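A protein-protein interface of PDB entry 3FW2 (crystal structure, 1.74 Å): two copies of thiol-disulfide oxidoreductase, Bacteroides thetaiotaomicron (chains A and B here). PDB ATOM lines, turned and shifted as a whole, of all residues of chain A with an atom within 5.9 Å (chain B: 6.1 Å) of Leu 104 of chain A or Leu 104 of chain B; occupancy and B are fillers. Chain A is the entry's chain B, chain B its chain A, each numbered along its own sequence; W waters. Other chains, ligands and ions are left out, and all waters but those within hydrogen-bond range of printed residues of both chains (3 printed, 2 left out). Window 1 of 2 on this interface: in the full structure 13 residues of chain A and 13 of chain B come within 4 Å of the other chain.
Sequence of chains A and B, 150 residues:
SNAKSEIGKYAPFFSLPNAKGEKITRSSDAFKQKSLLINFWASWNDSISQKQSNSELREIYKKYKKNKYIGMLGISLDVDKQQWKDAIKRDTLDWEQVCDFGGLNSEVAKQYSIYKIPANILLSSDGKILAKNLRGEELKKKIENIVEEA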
ATOM      1  N   TRP A  44      -0.650 -10.449  -8.540  1.00  0.00           N
ATOM      2  CA  TRP A  44       0.181 -11.262  -7.677  1.00  0.00           C
ATOM      3  C   TRP A  44       1.377 -11.912  -8.373  1.00  0.00           C
ATOM      4  O   TRP A  44       2.249 -12.449  -7.698  1.00  0.00           O
ATOM      5  CB  TRP A  44      -0.634 -12.331  -6.960  1.00  0.00           C
ATOM      6  CG  TRP A  44      -1.515 -13.241  -7.775  1.00  0.00           C
ATOM      7  CD1 TRP A  44      -2.849 -13.194  -7.856  1.00  0.00           C
ATOM      8  CD2 TRP A  44      -1.109 -14.344  -8.616  1.00  0.00           C
ATOM      9  NE1 TRP A  44      -3.335 -14.170  -8.662  1.00  0.00           N
ATOM     10  CE2 TRP A  44      -2.281 -14.906  -9.140  1.00  0.00           C
ATOM     11  CE3 TRP A  44       0.124 -14.924  -8.943  1.00  0.00           C
ATOM     12  CZ2 TRP A  44      -2.282 -15.982 -10.022  1.00  0.00           C
ATOM     13  CZ3 TRP A  44       0.114 -16.013  -9.834  1.00  0.00           C
ATOM     14  CH2 TRP A  44      -1.045 -16.537 -10.339  1.00  0.00           C
ATOM     15  N   LEU A  77      -6.390 -12.340 -13.881  1.00  0.00           N
ATOM     16  CA  LEU A  77      -6.758 -13.571 -13.197  1.00  0.00           C
ATOM     17  C   LEU A  77      -6.677 -13.369 -11.655  1.00  0.00           C
ATOM     18  O   LEU A  77      -6.681 -14.307 -10.867  1.00  0.00           O
ATOM     19  CB  LEU A  77      -5.912 -14.751 -13.677  1.00  0.00           C
ATOM     20  CG  LEU A  77      -6.140 -14.994 -15.191  1.00  0.00           C
ATOM     21  CD1 LEU A  77      -5.284 -16.245 -15.536  1.00  0.00           C
ATOM     22  CD2 LEU A  77      -7.649 -15.131 -15.640  1.00  0.00           C
ATOM     23  N   VAL A  79      -8.053 -12.460  -7.905  1.00  0.00           N
ATOM     24  CA  VAL A  79      -9.245 -12.670  -7.078  1.00  0.00           C
ATOM     25  C   VAL A  79      -9.522 -11.469  -6.147  1.00  0.00           C
ATOM     26  O   VAL A  79     -10.593 -11.376  -5.591  1.00  0.00           O
ATOM     27  CB  VAL A  79      -9.163 -13.958  -6.246  1.00  0.00           C
ATOM     28  CG1 VAL A  79      -9.150 -15.183  -7.215  1.00  0.00           C
ATOM     29  CG2 VAL A  79      -7.952 -13.976  -5.291  1.00  0.00           C
ATOM     30  N   GLY A 102     -12.547 -14.432 -10.605  1.00  0.00           N
ATOM     31  CA  GLY A 102     -12.681 -15.894 -10.566  1.00  0.00           C
ATOM     32  C   GLY A 102     -11.363 -16.633 -10.370  1.00  0.00           C
ATOM     33  O   GLY A 102     -11.339 -17.779  -9.913  1.00  0.00           O
ATOM     34  N   GLY A 103     -10.274 -15.978 -10.758  1.00  0.00           N
ATOM     35  CA  GLY A 103      -8.930 -16.462 -10.550  1.00  0.00           C
ATOM     36  C   GLY A 103      -8.436 -17.385 -11.671  1.00  0.00           C
ATOM     37  O   GLY A 103      -8.944 -17.409 -12.798  1.00  0.00           O
ATOM     38  N   LEU A 104      -7.478 -18.207 -11.318  1.00  0.00           N
ATOM     39  CA  LEU A 104      -6.779 -19.029 -12.308  1.00  0.00           C
ATOM     40  C   LEU A 104      -7.619 -20.079 -13.017  1.00  0.00           C
ATOM     41  O   LEU A 104      -7.305 -20.372 -14.179  1.00  0.00           O
ATOM     42  CB  LEU A 104      -5.574 -19.738 -11.688  1.00  0.00           C
ATOM     43  CG  LEU A 104      -4.368 -18.828 -11.397  1.00  0.00           C
ATOM     44  CD1 LEU A 104      -3.335 -19.678 -10.687  1.00  0.00           C
ATOM     45  CD2 LEU A 104      -3.710 -18.249 -12.642  1.00  0.00           C
ATOM     46  N   ASN A 105      -8.567 -20.644 -12.322  1.00  0.00           N
ATOM     47  CA  ASN A 105      -9.433 -21.732 -12.848  1.00  0.00           C
ATOM     48  C   ASN A 105     -10.720 -21.194 -13.446  1.00  0.00           C
ATOM     49  O   ASN A 105     -11.647 -21.971 -13.666  1.00  0.00           O
ATOM     50  CB  ASN A 105      -9.765 -22.738 -11.718  1.00  0.00           C
ATOM     51  CG  ASN A 105     -10.095 -24.172 -12.228  1.00  0.00           C
ATOM     52  OD1 ASN A 105      -9.525 -24.647 -13.194  1.00  0.00           O
ATOM     53  ND2 ASN A 105     -10.997 -24.861 -11.519  1.00  0.00           N
ATOM     54  N   SER A 106     -10.809 -19.889 -13.713  1.00  0.00           N
ATOM     55  CA  SER A 106     -12.073 -19.354 -14.213  1.00  0.00           C
ATOM     56  C   SER A 106     -12.239 -19.615 -15.696  1.00  0.00           C
ATOM     57  O   SER A 106     -11.308 -19.993 -16.399  1.00  0.00           O
ATOM     58  CB  SER A 106     -12.175 -17.828 -14.005  1.00  0.00           C
ATOM     59  OG  SER A 106     -11.114 -17.108 -14.628  1.00  0.00           O
ATOM     60  N   ALA A 109      -9.873 -18.239 -18.557  1.00  0.00           N
ATOM     61  CA  ALA A 109      -8.519 -18.872 -18.548  1.00  0.00           C
ATOM     62  C   ALA A 109      -8.542 -20.282 -19.158  1.00  0.00           C
ATOM     63  O   ALA A 109      -7.634 -20.710 -19.900  1.00  0.00           O
ATOM     64  CB  ALA A 109      -7.964 -18.900 -17.126  1.00  0.00           C
ATOM     65  N   LYS A 110      -9.614 -20.966 -18.848  1.00  0.00           N
ATOM     66  CA  LYS A 110      -9.838 -22.286 -19.429  1.00  0.00           C
ATOM     67  C   LYS A 110     -10.244 -22.158 -20.901  1.00  0.00           C
ATOM     68  O   LYS A 110      -9.679 -22.842 -21.710  1.00  0.00           O
ATOM     69  CB  LYS A 110     -10.805 -23.137 -18.580  1.00  0.00           C
ATOM     70  CG  LYS A 110     -12.280 -22.874 -18.725  1.00  0.00           C
ATOM     71  CD  LYS A 110     -13.144 -23.902 -17.962  1.00  0.00           C
ATOM     72  CE  LYS A 110     -13.136 -23.654 -16.430  1.00  0.00           C
ATOM     73  NZ  LYS A 110     -14.436 -24.127 -15.811  1.00  0.00           N
ATOM     74  N   ILE A 114      -4.872 -20.882 -21.303  1.00  0.00           N
ATOM     75  CA  ILE A 114      -3.736 -20.129 -20.727  1.00  0.00           C
ATOM     76  C   ILE A 114      -2.946 -21.147 -19.889  1.00  0.00           C
ATOM     77  O   ILE A 114      -3.498 -21.736 -18.988  1.00  0.00           O
ATOM     78  CB  ILE A 114      -4.251 -18.943 -19.911  1.00  0.00           C
ATOM     79  CG1 ILE A 114      -4.969 -17.921 -20.830  1.00  0.00           C
ATOM     80  CG2 ILE A 114      -3.065 -18.225 -19.160  1.00  0.00           C
ATOM     81  CD1 ILE A 114      -4.265 -17.586 -22.101  1.00  0.00           C
ATOM     82  N   TYR A 115      -1.670 -21.374 -20.196  1.00  0.00           N
ATOM     83  CA  TYR A 115      -0.926 -22.379 -19.416  1.00  0.00           C
ATOM     84  C   TYR A 115       0.001 -21.724 -18.401  1.00  0.00           C
ATOM     85  O   TYR A 115       0.374 -22.366 -17.424  1.00  0.00           O
ATOM     86  CB  TYR A 115      -0.140 -23.292 -20.306  1.00  0.00           C
ATOM     87  CG  TYR A 115       0.724 -22.611 -21.338  1.00  0.00           C
ATOM     88  CD1 TYR A 115       2.038 -22.271 -21.070  1.00  0.00           C
ATOM     89  CD2 TYR A 115       0.234 -22.377 -22.646  1.00  0.00           C
ATOM     90  CE1 TYR A 115       2.853 -21.688 -22.050  1.00  0.00           C
ATOM     91  CE2 TYR A 115       1.041 -21.774 -23.614  1.00  0.00           C
ATOM     92  CZ  TYR A 115       2.332 -21.430 -23.307  1.00  0.00           C
ATOM     93  OH  TYR A 115       3.133 -20.851 -24.253  1.00  0.00           O
ATOM     94  N   LYS A 116       0.256 -20.444 -18.583  1.00  0.00           N
ATOM     95  CA  LYS A 116       0.979 -19.627 -17.592  1.00  0.00           C
ATOM     96  C   LYS A 116       0.678 -18.157 -17.861  1.00  0.00           C
ATOM     97  O   LYS A 116       0.113 -17.813 -18.915  1.00  0.00           O
ATOM     98  CB  LYS A 116       2.475 -19.895 -17.667  1.00  0.00           C
ATOM     99  CG  LYS A 116       3.184 -19.334 -18.863  1.00  0.00           C
ATOM    100  CD  LYS A 116       4.709 -19.426 -18.665  1.00  0.00           C
ATOM    101  CE  LYS A 116       5.381 -19.758 -19.967  1.00  0.00           C
ATOM    102  NZ  LYS A 116       5.124 -18.674 -20.939  1.00  0.00           N
ATOM    103  N   ILE A 117       1.031 -17.283 -16.918  1.00  0.00           N
ATOM    104  CA  ILE A 117       0.916 -15.871 -17.125  1.00  0.00           C
ATOM    105  C   ILE A 117       2.331 -15.252 -16.941  1.00  0.00           C
ATOM    106  O   ILE A 117       3.190 -15.796 -16.231  1.00  0.00           O
ATOM    107  CB  ILE A 117      -0.096 -15.164 -16.214  1.00  0.00           C
ATOM    108  CG1 ILE A 117       0.018 -15.619 -14.758  1.00  0.00           C
ATOM    109  CG2 ILE A 117      -1.508 -15.406 -16.734  1.00  0.00           C
ATOM    110  CD1 ILE A 117      -0.844 -14.780 -13.774  1.00  0.00           C
ATOM    111  N   TRP B  44       7.789 -19.890 -12.841  1.00  0.00           N
ATOM    112  CA  TRP B  44       7.372 -18.698 -13.551  1.00  0.00           C
ATOM    113  C   TRP B  44       6.606 -17.680 -12.664  1.00  0.00           C
ATOM    114  O   TRP B  44       6.166 -16.590 -13.159  1.00  0.00           O
ATOM    115  CB  TRP B  44       6.547 -19.074 -14.805  1.00  0.00           C
ATOM    116  CG  TRP B  44       5.308 -19.929 -14.614  1.00  0.00           C
ATOM    117  CD1 TRP B  44       5.190 -21.255 -14.911  1.00  0.00           C
ATOM    118  CD2 TRP B  44       4.027 -19.508 -14.144  1.00  0.00           C
ATOM    119  NE1 TRP B  44       3.916 -21.677 -14.654  1.00  0.00           N
ATOM    120  CE2 TRP B  44       3.180 -20.622 -14.187  1.00  0.00           C
ATOM    121  CE3 TRP B  44       3.499 -18.274 -13.700  1.00  0.00           C
ATOM    122  CZ2 TRP B  44       1.827 -20.573 -13.779  1.00  0.00           C
ATOM    123  CZ3 TRP B  44       2.136 -18.236 -13.294  1.00  0.00           C
ATOM    124  CH2 TRP B  44       1.336 -19.374 -13.327  1.00  0.00           C
ATOM    125  N   LEU B  77       3.208 -25.929 -11.138  1.00  0.00           N
ATOM    126  CA  LEU B  77       2.457 -25.614 -12.342  1.00  0.00           C
ATOM    127  C   LEU B  77       3.361 -25.074 -13.454  1.00  0.00           C
ATOM    128  O   LEU B  77       2.904 -24.393 -14.392  1.00  0.00           O
ATOM    129  CB  LEU B  77       1.285 -24.676 -12.015  1.00  0.00           C
ATOM    130  CG  LEU B  77       0.373 -25.209 -10.923  1.00  0.00           C
ATOM    131  CD1 LEU B  77      -0.722 -24.166 -10.681  1.00  0.00           C
ATOM    132  CD2 LEU B  77      -0.236 -26.597 -11.242  1.00  0.00           C
ATOM    133  N   VAL B  79       5.572 -25.300 -16.896  1.00  0.00           N
ATOM    134  CA  VAL B  79       5.441 -25.954 -18.214  1.00  0.00           C
ATOM    135  C   VAL B  79       6.768 -26.390 -18.770  1.00  0.00           C
ATOM    136  O   VAL B  79       6.814 -27.229 -19.695  1.00  0.00           O
ATOM    137  CB  VAL B  79       4.775 -25.039 -19.214  1.00  0.00           C
ATOM    138  CG1 VAL B  79       3.255 -24.866 -18.807  1.00  0.00           C
ATOM    139  CG2 VAL B  79       5.561 -23.748 -19.365  1.00  0.00           C
ATOM    140  N   GLY B 102       1.753 -29.625 -17.410  1.00  0.00           N
ATOM    141  CA  GLY B 102       0.506 -29.106 -18.013  1.00  0.00           C
ATOM    142  C   GLY B 102       0.261 -27.630 -17.687  1.00  0.00           C
ATOM    143  O   GLY B 102      -0.604 -26.997 -18.277  1.00  0.00           O
ATOM    144  N   GLY B 103       0.980 -27.102 -16.696  1.00  0.00           N
ATOM    145  CA  GLY B 103       0.767 -25.711 -16.303  1.00  0.00           C
ATOM    146  C   GLY B 103      -0.559 -25.423 -15.675  1.00  0.00           C
ATOM    147  O   GLY B 103      -1.117 -26.244 -14.925  1.00  0.00           O
ATOM    148  N   LEU B 104      -1.152 -24.250 -15.973  1.00  0.00           N
ATOM    149  CA  LEU B 104      -2.508 -23.997 -15.530  1.00  0.00           C
ATOM    150  C   LEU B 104      -3.527 -24.954 -16.116  1.00  0.00           C
ATOM    151  O   LEU B 104      -4.621 -25.038 -15.642  1.00  0.00           O
ATOM    152  CB  LEU B 104      -2.940 -22.557 -15.852  1.00  0.00           C
ATOM    153  CG  LEU B 104      -2.010 -21.592 -15.160  1.00  0.00           C
ATOM    154  CD1 LEU B 104      -2.253 -20.075 -15.651  1.00  0.00           C
ATOM    155  CD2 LEU B 104      -1.950 -21.706 -13.638  1.00  0.00           C
ATOM    156  N   ASN B 105      -3.169 -25.670 -17.182  1.00  0.00           N
ATOM    157  CA  ASN B 105      -4.037 -26.729 -17.743  1.00  0.00           C
ATOM    158  C   ASN B 105      -3.763 -28.115 -17.081  1.00  0.00           C
ATOM    159  O   ASN B 105      -4.332 -29.125 -17.503  1.00  0.00           O
ATOM    160  CB  ASN B 105      -3.826 -26.789 -19.278  1.00  0.00           C
ATOM    161  CG  ASN B 105      -4.171 -25.460 -20.009  1.00  0.00           C
ATOM    162  OD1 ASN B 105      -5.136 -24.757 -19.644  1.00  0.00           O
ATOM    163  ND2 ASN B 105      -3.350 -25.103 -21.045  1.00  0.00           N
ATOM    164  N   SER B 106      -2.833 -28.211 -16.141  1.00  0.00           N
ATOM    165  CA  SER B 106      -2.555 -29.445 -15.368  1.00  0.00           C
ATOM    166  C   SER B 106      -3.849 -29.898 -14.673  1.00  0.00           C
ATOM    167  O   SER B 106      -4.527 -29.098 -13.986  1.00  0.00           O
ATOM    168  CB  SER B 106      -1.448 -29.216 -14.302  1.00  0.00           C
ATOM    169  OG  SER B 106      -0.868 -30.428 -13.756  1.00  0.00           O
ATOM    170  N   ALA B 109      -4.488 -28.952 -11.034  1.00  0.00           N
ATOM    171  CA  ALA B 109      -4.846 -27.553 -10.762  1.00  0.00           C
ATOM    172  C   ALA B 109      -6.331 -27.318 -10.817  1.00  0.00           C
ATOM    173  O   ALA B 109      -6.871 -26.550 -10.041  1.00  0.00           O
ATOM    174  CB  ALA B 109      -4.113 -26.586 -11.745  1.00  0.00           C
ATOM    175  N   LYS B 110      -6.987 -27.968 -11.764  1.00  0.00           N
ATOM    176  CA  LYS B 110      -8.417 -27.910 -11.863  1.00  0.00           C
ATOM    177  C   LYS B 110      -9.037 -28.700 -10.738  1.00  0.00           C
ATOM    178  O   LYS B 110     -10.018 -28.243 -10.113  1.00  0.00           O
ATOM    179  CB  LYS B 110      -8.844 -28.459 -13.220  1.00  0.00           C
ATOM    180  CG  LYS B 110      -8.156 -27.748 -14.383  1.00  0.00           C
ATOM    181  CD  LYS B 110      -8.681 -28.200 -15.761  1.00  0.00           C
ATOM    182  CE  LYS B 110      -7.812 -29.268 -16.364  1.00  0.00           C
ATOM    183  NZ  LYS B 110      -8.373 -29.834 -17.643  1.00  0.00           N
ATOM    184  N   ILE B 114      -7.308 -24.494  -7.840  1.00  0.00           N
ATOM    185  CA  ILE B 114      -6.221 -23.552  -7.487  1.00  0.00           C
ATOM    186  C   ILE B 114      -6.541 -22.227  -8.177  1.00  0.00           C
ATOM    187  O   ILE B 114      -6.626 -22.134  -9.440  1.00  0.00           O
ATOM    188  CB  ILE B 114      -4.865 -24.120  -7.912  1.00  0.00           C
ATOM    189  CG1 ILE B 114      -4.618 -25.438  -7.202  1.00  0.00           C
ATOM    190  CG2 ILE B 114      -3.704 -23.158  -7.604  1.00  0.00           C
ATOM    191  CD1 ILE B 114      -4.587 -25.398  -5.675  1.00  0.00           C
ATOM    192  N   TYR B 115      -6.822 -21.199  -7.369  1.00  0.00           N
ATOM    193  CA  TYR B 115      -7.201 -19.942  -7.945  1.00  0.00           C
ATOM    194  C   TYR B 115      -6.081 -18.931  -7.987  1.00  0.00           C
ATOM    195  O   TYR B 115      -6.178 -17.927  -8.686  1.00  0.00           O
ATOM    196  CB  TYR B 115      -8.419 -19.373  -7.215  1.00  0.00           C
ATOM    197  CG  TYR B 115      -8.248 -19.149  -5.753  1.00  0.00           C
ATOM    198  CD1 TYR B 115      -7.610 -17.996  -5.266  1.00  0.00           C
ATOM    199  CD2 TYR B 115      -8.767 -20.070  -4.818  1.00  0.00           C
ATOM    200  CE1 TYR B 115      -7.488 -17.767  -3.850  1.00  0.00           C
ATOM    201  CE2 TYR B 115      -8.601 -19.849  -3.433  1.00  0.00           C
ATOM    202  CZ  TYR B 115      -8.003 -18.708  -2.974  1.00  0.00           C
ATOM    203  OH  TYR B 115      -7.874 -18.474  -1.619  1.00  0.00           O
ATOM    204  N   LYS B 116      -5.036 -19.212  -7.225  1.00  0.00           N
ATOM    205  CA  LYS B 116      -3.823 -18.428  -7.223  1.00  0.00           C
ATOM    206  C   LYS B 116      -2.682 -19.275  -6.709  1.00  0.00           C
ATOM    207  O   LYS B 116      -2.900 -20.278  -5.994  1.00  0.00           O
ATOM    208  CB  LYS B 116      -4.001 -17.116  -6.421  1.00  0.00           C
ATOM    209  CG  LYS B 116      -3.970 -17.236  -4.928  1.00  0.00           C
ATOM    210  CD  LYS B 116      -3.999 -15.802  -4.140  1.00  0.00           C
ATOM    211  CE  LYS B 116      -3.046 -14.779  -4.735  1.00  0.00           C
ATOM    212  NZ  LYS B 116      -2.338 -13.763  -3.770  1.00  0.00           N
ATOM    213  N   ILE B 117      -1.440 -18.872  -7.030  1.00  0.00           N
ATOM    214  CA  ILE B 117      -0.268 -19.485  -6.385  1.00  0.00           C
ATOM    215  C   ILE B 117       0.569 -18.405  -5.754  1.00  0.00           C
ATOM    216  O   ILE B 117       0.571 -17.270  -6.217  1.00  0.00           O
ATOM    217  CB  ILE B 117       0.572 -20.364  -7.336  1.00  0.00           C
ATOM    218  CG1 ILE B 117       0.779 -19.621  -8.675  1.00  0.00           C
ATOM    219  CG2 ILE B 117      -0.109 -21.735  -7.511  1.00  0.00           C
ATOM    220  CD1 ILE B 117       1.871 -20.247  -9.634  1.00  0.00           C
HETATM  221  O   HOH W   1       2.357 -14.819  -5.945  1.00  0.00           O
HETATM  222  O   HOH W   2      -5.793 -15.159  -8.626  1.00  0.00           O
HETATM  223  O   HOH W   3       5.631 -15.169 -15.188  1.00  0.00           O
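O of Ile 117 of chain B touches CE3 of Trp 44 of chain A (3.6 Å).
Val 79 of chain A touches Tyr 115 of chain B.
Leu 104 of chain A touches Leu 104 of chain B.
Leu 104 of chain A touches Ile 114 of chain B (CB to O, 3.4 Å).
Leu 104 of chain A touches Lys 116 of chain B (CD1 to CA, 3.7 Å).
CG of Lys 110 of chain B touches OD1 of Asn 105 of chain A (3.6 Å).
Ile 114 of chain A touches Leu 104 of chain B.
Tyr 115 of chain A touches Val 79 of chain B.
Gly 103 of chain B touches Tyr 115 of chain A.
CA of Lys 116 of chain A touches CD1 of Leu 104 of chain B, 3.8 Å away.
O of Tyr 115 of chain A sits at hydrogen-bond distance from N of Leu 104 of chain B, 2.8 Å away.
The backbone carbonyl oxygen (O) of Tyr 115 of chain B sits at hydrogen-bond distance from the backbone NH (N) of Leu 104 of chain A, at 2.9 Å.
OD1 of Asn 105 of chain B sits close to O of Ile 114 of chain A (3.5 Å).
Of chain B, only Leu 104, Ile 114, Tyr 115 and Lys 116 come within 4 Å of Leu 104 of chain A.
Of the printed residues of chain A, Leu 104 of chain B touches Leu 104, Ile 114, Tyr 115 and Lys 116.
Of the printed residues of chain B, Trp 44 of chain A touches Lys 116 (3.5 Å) and Ile 117 (3.6 Å).
Of the printed residues of chain A, Ile 114 of chain B touches Leu 104 (3.4 Å) and Asn 105 (3.8 Å).
Of the printed residues of chain B, Val 79 of chain A touches Tyr 115 (3.8 Å).
Ala 109 of chain A touches none of the printed residues of chain B.
Leu 77 of chain A touches none of the printed residues of chain B.
The nearest residue of chain B that does not touch Leu 104 of chain A is Ile 117 of chain B (4.2 Å).
The nearest printed residue of chain A that does not touch Leu 104 of chain B is Ile 117 of chain A (4.5 Å).
Of the 14 printed residues of chain B, 10 touch a printed residue of chain A.
Hydrophobic or aromatic side chains of chain B within 4 Å of the printed part of chain A: Trp 44, Val 79, Leu 104, Tyr 115 and Ile 117.
Of the 14 printed residues of chain A, 9 touch a printed residue of chain B.
Printed residues of chain A that touch a printed residue of chain B: Trp 44, Val 79, Gly 103, Leu 104, Asn 105, Ile 114, Tyr 115, Lys 116 and Ile 117.
Hydrophobic or aromatic side chains of chain A that line the printed part of chain B: Trp 44, Val 79, Leu 104, Tyr 115 and Ile 117.
Among the printed residues, 19 pairs touch across the chains.
Among the printed residues, no Asp or Glu carboxylate lies within 4 Å of a Lys or Arg side-chain nitrogen of the other chain.
Leu 104 of chain B touches its own counterpart, Leu 104 of chain A.
Leu 104 of chain A touches Tyr 115 of chain B, and with the chains exchanged Tyr 115 of chain A touches Leu 104 of chain B.
Asn 105 of chain A touches Lys 110 of chain B, but with the chains exchanged Lys 110 of chain A does not touch Asn 105 of chain B (5.3 Å).
Tyr 115 of chain A touches Asn 105 of chain B, but with the chains exchanged Asn 105 of chain A does not touch Tyr 115 of chain B (4.6 Å).
Positions printed for both chains: 44, 77, 79, 102, 103, 104, 105, 106, 109, 110, 114, 115, 116 and 117.
O of Ala 109 of chain A lies within hydrogen-bond range of N of Ile 114 of chain A (3.1 Å).
NE1 of Trp 44 of chain B sits at hydrogen-bond distance from O of Leu 77 of chain B (2.9 Å).
O of Gly 103 of chain A sits at hydrogen-bond distance from OG of Ser 106 of chain A, 2.9 Å away.
The backbone carbonyl oxygen (O) of Ala 109 of chain B lies within hydrogen-bond range of the backbone NH (N) of Ile 114 of chain B (3.0 Å).
Water W3 bridges O of Trp 44 of chain B (2.5 Å) and O of Ile 117 of chain A (2.7 Å).
Water W2 lies within hydrogen-bond range of the backbone carbonyl oxygen of Leu 77 of chain A, the indole nitrogen of Trp 44 of chain A and the backbone carbonyl oxygen of Tyr 115 of chain B.
Water W1 lies within hydrogen-bond range of the backbone carbonyl oxygen of Trp 44 of chain A (2.9 Å) and the backbone carbonyl oxygen of Ile 117 of chain B (3.0 Å).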
